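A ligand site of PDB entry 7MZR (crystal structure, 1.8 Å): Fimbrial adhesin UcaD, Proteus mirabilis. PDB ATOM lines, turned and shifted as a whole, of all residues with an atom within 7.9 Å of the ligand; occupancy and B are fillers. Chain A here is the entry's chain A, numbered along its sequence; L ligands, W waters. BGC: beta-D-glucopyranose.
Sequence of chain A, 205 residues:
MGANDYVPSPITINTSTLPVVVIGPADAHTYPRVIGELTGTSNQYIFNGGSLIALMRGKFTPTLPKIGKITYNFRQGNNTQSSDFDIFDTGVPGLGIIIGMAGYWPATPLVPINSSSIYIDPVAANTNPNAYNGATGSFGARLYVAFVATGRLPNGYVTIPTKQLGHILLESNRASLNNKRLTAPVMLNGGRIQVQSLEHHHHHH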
ATOM      1  N   ASN A  43      10.765  14.165 -20.752  1.00  0.00           N
ATOM      2  CA  ASN A  43      11.872  13.288 -20.359  1.00  0.00           C
ATOM      3  C   ASN A  43      12.303  13.734 -18.969  1.00  0.00           C
ATOM      4  O   ASN A  43      12.736  14.877 -18.792  1.00  0.00           O
ATOM      5  CB  ASN A  43      13.001  13.362 -21.371  1.00  0.00           C
ATOM      6  CG  ASN A  43      14.137  12.421 -21.043  1.00  0.00           C
ATOM      7  OD1 ASN A  43      14.197  11.893 -19.946  1.00  0.00           O
ATOM      8  ND2 ASN A  43      15.044  12.236 -21.987  1.00  0.00           N
ATOM      9  N   GLN A  44      12.112  12.857 -17.992  1.00  0.00           N
ATOM     10  CA  GLN A  44      12.473  13.186 -16.612  1.00  0.00           C
ATOM     11  C   GLN A  44      13.979  13.246 -16.413  1.00  0.00           C
ATOM     12  O   GLN A  44      14.436  13.909 -15.456  1.00  0.00           O
ATOM     13  CB  GLN A  44      11.851  12.150 -15.668  1.00  0.00           C
ATOM     14  CG  GLN A  44      12.012  12.484 -14.214  1.00  0.00           C
ATOM     15  CD  GLN A  44      11.282  11.529 -13.286  1.00  0.00           C
ATOM     16  OE1 GLN A  44      10.543  10.642 -13.737  1.00  0.00           O
ATOM     17  NE2 GLN A  44      11.448  11.728 -12.005  1.00  0.00           N
ATOM     18  N   TYR A  45      14.756  12.624 -17.295  1.00  0.00           N
ATOM     19  CA  TYR A  45      16.192  12.420 -17.088  1.00  0.00           C
ATOM     20  C   TYR A  45      16.988  12.908 -18.287  1.00  0.00           C
ATOM     21  O   TYR A  45      17.767  12.181 -18.895  1.00  0.00           O
ATOM     22  CB  TYR A  45      16.450  10.936 -16.799  1.00  0.00           C
ATOM     23  CG  TYR A  45      15.640  10.414 -15.639  1.00  0.00           C
ATOM     24  CD1 TYR A  45      15.916  10.835 -14.340  1.00  0.00           C
ATOM     25  CD2 TYR A  45      14.626   9.481 -15.824  1.00  0.00           C
ATOM     26  CE1 TYR A  45      15.166  10.366 -13.255  1.00  0.00           C
ATOM     27  CE2 TYR A  45      13.878   8.997 -14.733  1.00  0.00           C
ATOM     28  CZ  TYR A  45      14.164   9.451 -13.465  1.00  0.00           C
ATOM     29  OH  TYR A  45      13.434   8.988 -12.387  1.00  0.00           O
ATOM     30  N   ILE A  46      16.791  14.196 -18.624  1.00  0.00           N
ATOM     31  CA  ILE A  46      17.633  14.803 -19.661  1.00  0.00           C
ATOM     32  C   ILE A  46      19.074  14.892 -19.174  1.00  0.00           C
ATOM     33  O   ILE A  46      20.018  14.621 -19.923  1.00  0.00           O
ATOM     34  CB  ILE A  46      17.069  16.167 -20.068  1.00  0.00           C
ATOM     35  CG1 ILE A  46      15.696  15.960 -20.715  1.00  0.00           C
ATOM     36  CG2 ILE A  46      18.017  16.870 -21.010  1.00  0.00           C
ATOM     37  CD1 ILE A  46      14.961  17.257 -21.103  1.00  0.00           C
ATOM     38  N   PHE A  47      19.288  15.263 -17.910  1.00  0.00           N
ATOM     39  CA  PHE A  47      20.590  15.128 -17.264  1.00  0.00           C
ATOM     40  C   PHE A  47      20.433  14.255 -16.030  1.00  0.00           C
ATOM     41  O   PHE A  47      19.519  14.468 -15.230  1.00  0.00           O
ATOM     42  CB  PHE A  47      21.176  16.498 -16.900  1.00  0.00           C
ATOM     43  CG  PHE A  47      21.341  17.409 -18.084  1.00  0.00           C
ATOM     44  CD1 PHE A  47      22.386  17.223 -18.987  1.00  0.00           C
ATOM     45  CD2 PHE A  47      20.459  18.433 -18.277  1.00  0.00           C
ATOM     46  CE1 PHE A  47      22.510  18.033 -20.079  1.00  0.00           C
ATOM     47  CE2 PHE A  47      20.596  19.260 -19.358  1.00  0.00           C
ATOM     48  CZ  PHE A  47      21.636  19.053 -20.266  1.00  0.00           C
ATOM     49  N   ASN A  48      21.315  13.276 -15.884  1.00  0.00           N
ATOM     50  CA  ASN A  48      21.154  12.311 -14.799  1.00  0.00           C
ATOM     51  C   ASN A  48      22.461  11.547 -14.632  1.00  0.00           C
ATOM     52  O   ASN A  48      23.207  11.389 -15.604  1.00  0.00           O
ATOM     53  CB  ASN A  48      20.005  11.334 -15.118  1.00  0.00           C
ATOM     54  CG  ASN A  48      19.653  10.415 -13.965  1.00  0.00           C
ATOM     55  OD1 ASN A  48      19.783  10.766 -12.799  1.00  0.00           O
ATOM     56  ND2 ASN A  48      19.140   9.232 -14.297  1.00  0.00           N
ATOM     57  N   ALA A  54      22.610  18.296  -6.983  1.00  0.00           N
ATOM     58  CA  ALA A  54      23.022  19.613  -7.427  1.00  0.00           C
ATOM     59  C   ALA A  54      21.787  20.473  -7.659  1.00  0.00           C
ATOM     60  O   ALA A  54      20.700  19.975  -7.965  1.00  0.00           O
ATOM     61  CB  ALA A  54      23.842  19.537  -8.725  1.00  0.00           C
ATOM     62  N   MET A  56      20.380  22.826 -10.277  1.00  0.00           N
ATOM     63  CA  MET A  56      20.555  22.826 -11.727  1.00  0.00           C
ATOM     64  C   MET A  56      19.486  23.664 -12.395  1.00  0.00           C
ATOM     65  O   MET A  56      18.413  23.923 -11.844  1.00  0.00           O
ATOM     66  CB  MET A  56      20.536  21.383 -12.280  1.00  0.00           C
ATOM     67  CG  MET A  56      21.734  20.539 -11.791  1.00  0.00           C
ATOM     68  SD  MET A  56      21.673  18.798 -12.284  1.00  0.00           S
ATOM     69  CE  MET A  56      20.532  18.081 -11.084  1.00  0.00           C
ATOM     70  N   ALA A 102       9.017  23.386 -20.717  1.00  0.00           N
ATOM     71  CA  ALA A 102       8.708  23.587 -19.317  1.00  0.00           C
ATOM     72  C   ALA A 102       9.577  22.656 -18.487  1.00  0.00           C
ATOM     73  O   ALA A 102      10.202  21.725 -19.000  1.00  0.00           O
ATOM     74  CB  ALA A 102       7.232  23.312 -19.011  1.00  0.00           C
ATOM     75  N   GLY A 103       9.595  22.924 -17.189  1.00  0.00           N
ATOM     76  CA  GLY A 103      10.114  21.937 -16.256  1.00  0.00           C
ATOM     77  C   GLY A 103       9.304  20.649 -16.308  1.00  0.00           C
ATOM     78  O   GLY A 103       8.194  20.575 -16.821  1.00  0.00           O
ATOM     79  N   TYR A 104       9.897  19.608 -15.750  1.00  0.00           N
ATOM     80  CA  TYR A 104       9.285  18.287 -15.852  1.00  0.00           C
ATOM     81  C   TYR A 104       7.953  18.231 -15.120  1.00  0.00           C
ATOM     82  O   TYR A 104       6.958  17.695 -15.648  1.00  0.00           O
ATOM     83  CB  TYR A 104      10.228  17.221 -15.299  1.00  0.00           C
ATOM     84  CG  TYR A 104       9.643  15.853 -15.472  1.00  0.00           C
ATOM     85  CD1 TYR A 104       9.565  15.293 -16.739  1.00  0.00           C
ATOM     86  CD2 TYR A 104       9.102  15.144 -14.418  1.00  0.00           C
ATOM     87  CE1 TYR A 104       8.993  14.082 -16.944  1.00  0.00           C
ATOM     88  CE2 TYR A 104       8.512  13.902 -14.615  1.00  0.00           C
ATOM     89  CZ  TYR A 104       8.458  13.385 -15.890  1.00  0.00           C
ATOM     90  OH  TYR A 104       7.890  12.161 -16.147  1.00  0.00           O
ATOM     91  N   TRP A 105       7.915  18.748 -13.919  1.00  0.00           N
ATOM     92  CA  TRP A 105       6.706  18.552 -13.137  1.00  0.00           C
ATOM     93  C   TRP A 105       5.595  19.473 -13.629  1.00  0.00           C
ATOM     94  O   TRP A 105       5.857  20.577 -14.104  1.00  0.00           O
ATOM     95  CB  TRP A 105       6.978  18.772 -11.656  1.00  0.00           C
ATOM     96  CG  TRP A 105       8.016  17.808 -11.140  1.00  0.00           C
ATOM     97  CD1 TRP A 105       9.260  18.123 -10.670  1.00  0.00           C
ATOM     98  CD2 TRP A 105       7.905  16.370 -11.072  1.00  0.00           C
ATOM     99  NE1 TRP A 105       9.930  16.988 -10.308  1.00  0.00           N
ATOM    100  CE2 TRP A 105       9.126  15.901 -10.526  1.00  0.00           C
ATOM    101  CE3 TRP A 105       6.908  15.446 -11.392  1.00  0.00           C
ATOM    102  CZ2 TRP A 105       9.375  14.542 -10.313  1.00  0.00           C
ATOM    103  CZ3 TRP A 105       7.157  14.104 -11.168  1.00  0.00           C
ATOM    104  CH2 TRP A 105       8.374  13.667 -10.633  1.00  0.00           C
ATOM    105  N   THR A 108       5.090  23.530 -13.300  1.00  0.00           N
ATOM    106  CA  THR A 108       5.954  24.547 -13.909  1.00  0.00           C
ATOM    107  C   THR A 108       5.364  24.969 -15.241  1.00  0.00           C
ATOM    108  O   THR A 108       4.818  24.141 -15.963  1.00  0.00           O
ATOM    109  CB  THR A 108       7.375  24.007 -14.131  1.00  0.00           C
ATOM    110  OG1 THR A 108       7.330  22.941 -15.069  1.00  0.00           O
ATOM    111  CG2 THR A 108       7.989  23.518 -12.841  1.00  0.00           C
ATOM    112  N   ASP A 121      13.601  26.151 -17.110  1.00  0.00           N
ATOM    113  CA  ASP A 121      13.303  25.750 -15.737  1.00  0.00           C
ATOM    114  C   ASP A 121      14.555  25.986 -14.890  1.00  0.00           C
ATOM    115  O   ASP A 121      15.642  25.496 -15.230  1.00  0.00           O
ATOM    116  CB  ASP A 121      12.865  24.293 -15.671  1.00  0.00           C
ATOM    117  CG  ASP A 121      12.303  23.900 -14.301  1.00  0.00           C
ATOM    118  OD1 ASP A 121      11.523  24.687 -13.728  1.00  0.00           O
ATOM    119  OD2 ASP A 121      12.638  22.804 -13.815  1.00  0.00           O
ATOM    120  N   ASN A 133      16.938  25.273  -9.880  1.00  0.00           N
ATOM    121  CA  ASN A 133      16.050  24.299  -9.263  1.00  0.00           C
ATOM    122  C   ASN A 133      16.570  23.904  -7.886  1.00  0.00           C
ATOM    123  O   ASN A 133      17.781  23.965  -7.630  1.00  0.00           O
ATOM    124  CB  ASN A 133      15.907  23.040 -10.104  1.00  0.00           C
ATOM    125  CG  ASN A 133      15.010  23.254 -11.304  1.00  0.00           C
ATOM    126  OD1 ASN A 133      14.279  24.229 -11.352  1.00  0.00           O
ATOM    127  ND2 ASN A 133      15.110  22.366 -12.285  1.00  0.00           N
ATOM    128  N   GLY A 134      15.656  23.495  -7.015  1.00  0.00           N
ATOM    129  CA  GLY A 134      16.076  22.899  -5.754  1.00  0.00           C
ATOM    130  C   GLY A 134      16.914  21.656  -5.984  1.00  0.00           C
ATOM    131  O   GLY A 134      16.800  20.992  -7.015  1.00  0.00           O
ATOM    132  N   ALA A 135      17.784  21.365  -5.024  1.00  0.00           N
ATOM    133  CA  ALA A 135      18.784  20.336  -5.223  1.00  0.00           C
ATOM    134  C   ALA A 135      18.146  18.975  -5.427  1.00  0.00           C
ATOM    135  O   ALA A 135      17.202  18.587  -4.727  1.00  0.00           O
ATOM    136  CB  ALA A 135      19.723  20.315  -4.017  1.00  0.00           C
ATOM    137  N   THR A 136      18.645  18.252  -6.418  1.00  0.00           N
ATOM    138  CA  THR A 136      18.196  16.886  -6.660  1.00  0.00           C
ATOM    139  C   THR A 136      19.186  16.216  -7.604  1.00  0.00           C
ATOM    140  O   THR A 136      20.272  16.754  -7.883  1.00  0.00           O
ATOM    141  CB  THR A 136      16.748  16.870  -7.165  1.00  0.00           C
ATOM    142  OG1 THR A 136      16.310  15.506  -7.268  1.00  0.00           O
ATOM    143  CG2 THR A 136      16.611  17.562  -8.518  1.00  0.00           C
ATOM    144  N   GLY A 137      18.858  15.010  -8.037  1.00  0.00           N
ATOM    145  CA  GLY A 137      19.768  14.191  -8.788  1.00  0.00           C
ATOM    146  C   GLY A 137      19.505  14.123 -10.278  1.00  0.00           C
ATOM    147  O   GLY A 137      20.133  13.330 -10.972  1.00  0.00           O
ATOM    148  N   SER A 138      18.592  14.941 -10.790  1.00  0.00           N
ATOM    149  CA  SER A 138      18.243  14.862 -12.198  1.00  0.00           C
ATOM    150  C   SER A 138      17.643  16.194 -12.648  1.00  0.00           C
ATOM    151  O   SER A 138      17.182  16.985 -11.823  1.00  0.00           O
ATOM    152  CB  SER A 138      17.256  13.702 -12.475  1.00  0.00           C
ATOM    153  OG  SER A 138      16.135  13.718 -11.610  1.00  0.00           O
ATOM    154  N   PHE A 139      17.655  16.404 -13.967  1.00  0.00           N
ATOM    155  CA  PHE A 139      16.964  17.527 -14.593  1.00  0.00           C
ATOM    156  C   PHE A 139      16.178  17.007 -15.786  1.00  0.00           C
ATOM    157  O   PHE A 139      16.751  16.356 -16.669  1.00  0.00           O
ATOM    158  CB  PHE A 139      17.949  18.612 -15.050  1.00  0.00           C
ATOM    159  CG  PHE A 139      17.273  19.765 -15.736  1.00  0.00           C
ATOM    160  CD1 PHE A 139      16.956  19.697 -17.088  1.00  0.00           C
ATOM    161  CD2 PHE A 139      16.918  20.875 -15.033  1.00  0.00           C
ATOM    162  CE1 PHE A 139      16.294  20.719 -17.727  1.00  0.00           C
ATOM    163  CE2 PHE A 139      16.275  21.928 -15.679  1.00  0.00           C
ATOM    164  CZ  PHE A 139      15.968  21.840 -17.021  1.00  0.00           C
ATOM    165  N   GLY A 140      14.874  17.260 -15.813  1.00  0.00           N
ATOM    166  CA  GLY A 140      14.038  16.885 -16.935  1.00  0.00           C
ATOM    167  C   GLY A 140      13.238  18.065 -17.455  1.00  0.00           C
ATOM    168  O   GLY A 140      13.349  19.188 -16.963  1.00  0.00           O
ATOM    169  N   ALA A 141      12.425  17.778 -18.475  1.00  0.00           N
ATOM    170  CA  ALA A 141      11.667  18.863 -19.101  1.00  0.00           C
ATOM    171  C   ALA A 141      10.500  18.278 -19.864  1.00  0.00           C
ATOM    172  O   ALA A 141      10.448  17.076 -20.134  1.00  0.00           O
ATOM    173  CB  ALA A 141      12.532  19.681 -20.073  1.00  0.00           C
HETATM  174  C2  BGC L   1      12.954  15.239 -11.481  1.00  0.00           C
HETATM  175  C3  BGC L   1      13.548  16.091 -12.600  1.00  0.00           C
HETATM  176  C4  BGC L   1      13.284  17.574 -12.343  1.00  0.00           C
HETATM  177  C5  BGC L   1      13.743  17.953 -10.943  1.00  0.00           C
HETATM  178  C6  BGC L   1      13.484  19.393 -10.570  1.00  0.00           C
HETATM  179  C1  BGC L   1      13.392  15.751 -10.115  1.00  0.00           C
HETATM  180  O1  BGC L   1      12.766  15.034  -9.071  1.00  0.00           O
HETATM  181  O2  BGC L   1      13.374  13.884 -11.618  1.00  0.00           O
HETATM  182  O3  BGC L   1      12.992  15.742 -13.854  1.00  0.00           O
HETATM  183  O4  BGC L   1      14.004  18.361 -13.291  1.00  0.00           O
HETATM  184  O5  BGC L   1      13.062  17.134  -9.980  1.00  0.00           O
HETATM  185  O6  BGC L   1      12.111  19.686 -10.448  1.00  0.00           O
HETATM  186  O   HOH W   1      10.339  20.517 -12.693  1.00  0.00           O
HETATM  187  O   HOH W   2      13.942  20.354  -7.271  1.00  0.00           O
HETATM  188  O   HOH W   3      13.848  15.291  -6.595  1.00  0.00           O
HETATM  189  O   HOH W   4      12.886  12.309  -8.929  1.00  0.00           O
HETATM  190  O   HOH W   5      10.991  19.042  -7.773  1.00  0.00           O
HETATM  191  O   HOH W   6      12.596  20.186 -14.605  1.00  0.00           O
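The side-chain hydroxyl (OG) of Ser 138 sits at hydrogen-bond distance from an oxygen (O2) of the ligand, 2.8 Å away.
The backbone carbonyl oxygen (O) of Gln 44 lies within hydrogen-bond range of an oxygen (O3) of the ligand, at 2.8 Å.
The side-chain amide nitrogen of Gln 44 sits at hydrogen-bond distance from an oxygen (O2) of the ligand (2.9 Å).
O4 of the ligand sits at hydrogen-bond distance from N of Gly 140 (2.9 Å).
The indole nitrogen (NE1) of Trp 105 lies within hydrogen-bond range of an oxygen (O5) of the ligand, 3.2 Å away.
O of Gln 44 sits close to N of Gly 140, 3.4 Å away.
The side-chain hydroxyl of Tyr 45 is in hydrogen-bond range of the side-chain amide nitrogen of Gln 44, 3.4 Å away.
O of Trp 105 lies within hydrogen-bond range of OG1 of Thr 108.
O of Phe 139 lies within hydrogen-bond range of N of Ile 46 (2.9 Å).
N of Phe 139 is in hydrogen-bond range of O of Phe 47.
N of Ala 54 is in hydrogen-bond range of O of Thr 136 (2.9 Å).
OD2 of Asp 121 lies within hydrogen-bond range of ND2 of Asn 133, at 2.9 Å.
The backbone NH (N) of Asn 133 sits at hydrogen-bond distance from the backbone carbonyl oxygen (O) of Met 56, at 2.8 Å.
Tyr 104 touches the ligand (CB to O3, 3.5 Å).
Asn 133 touches the ligand (ND2 to C6, 3.8 Å).
CG2 of Thr 136 touches C5 of the ligand (3.8 Å).
CA of Phe 139 touches O4 of the ligand (3.3 Å).
Hydrophobic or aromatic side chains that line the ligand: Tyr 104 and Trp 105.
Eight residues have an atom within 4 Å of the ligand: Gln 44, Tyr 104, Trp 105, Asn 133, Thr 136, Ser 138, Phe 139 and Gly 140.
The nearest printed residue that does not touch the ligand is Tyr 45 (4.3 Å).
Water W6 lies within hydrogen-bond range of an oxygen (O4) of the ligand (2.7 Å), the backbone carbonyl oxygen (O) of Gly 140 (2.7 Å), the side-chain carboxylate (OD2) of Asp 121 (2.7 Å) and the backbone NH (N) of Tyr 104 (3.0 Å).
Water W3 bridges OG1 of Thr 136 and O1 of the ligand.
Water W4 bridges an oxygen (O1) of the ligand (2.7 Å) and the side-chain amide nitrogen of Gln 44 (3.4 Å).
Water W5 bridges O6 of the ligand (3.0 Å) and NE1 of Trp 105 (3.4 Å).
Water W1 lies within hydrogen-bond range of an oxygen (O6) of the ligand (3.0 Å), the backbone NH of Tyr 104 (3.2 Å), the backbone NH of Trp 105 (3.2 Å) and the side-chain carboxylate of Asp 121 (3.4 Å).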
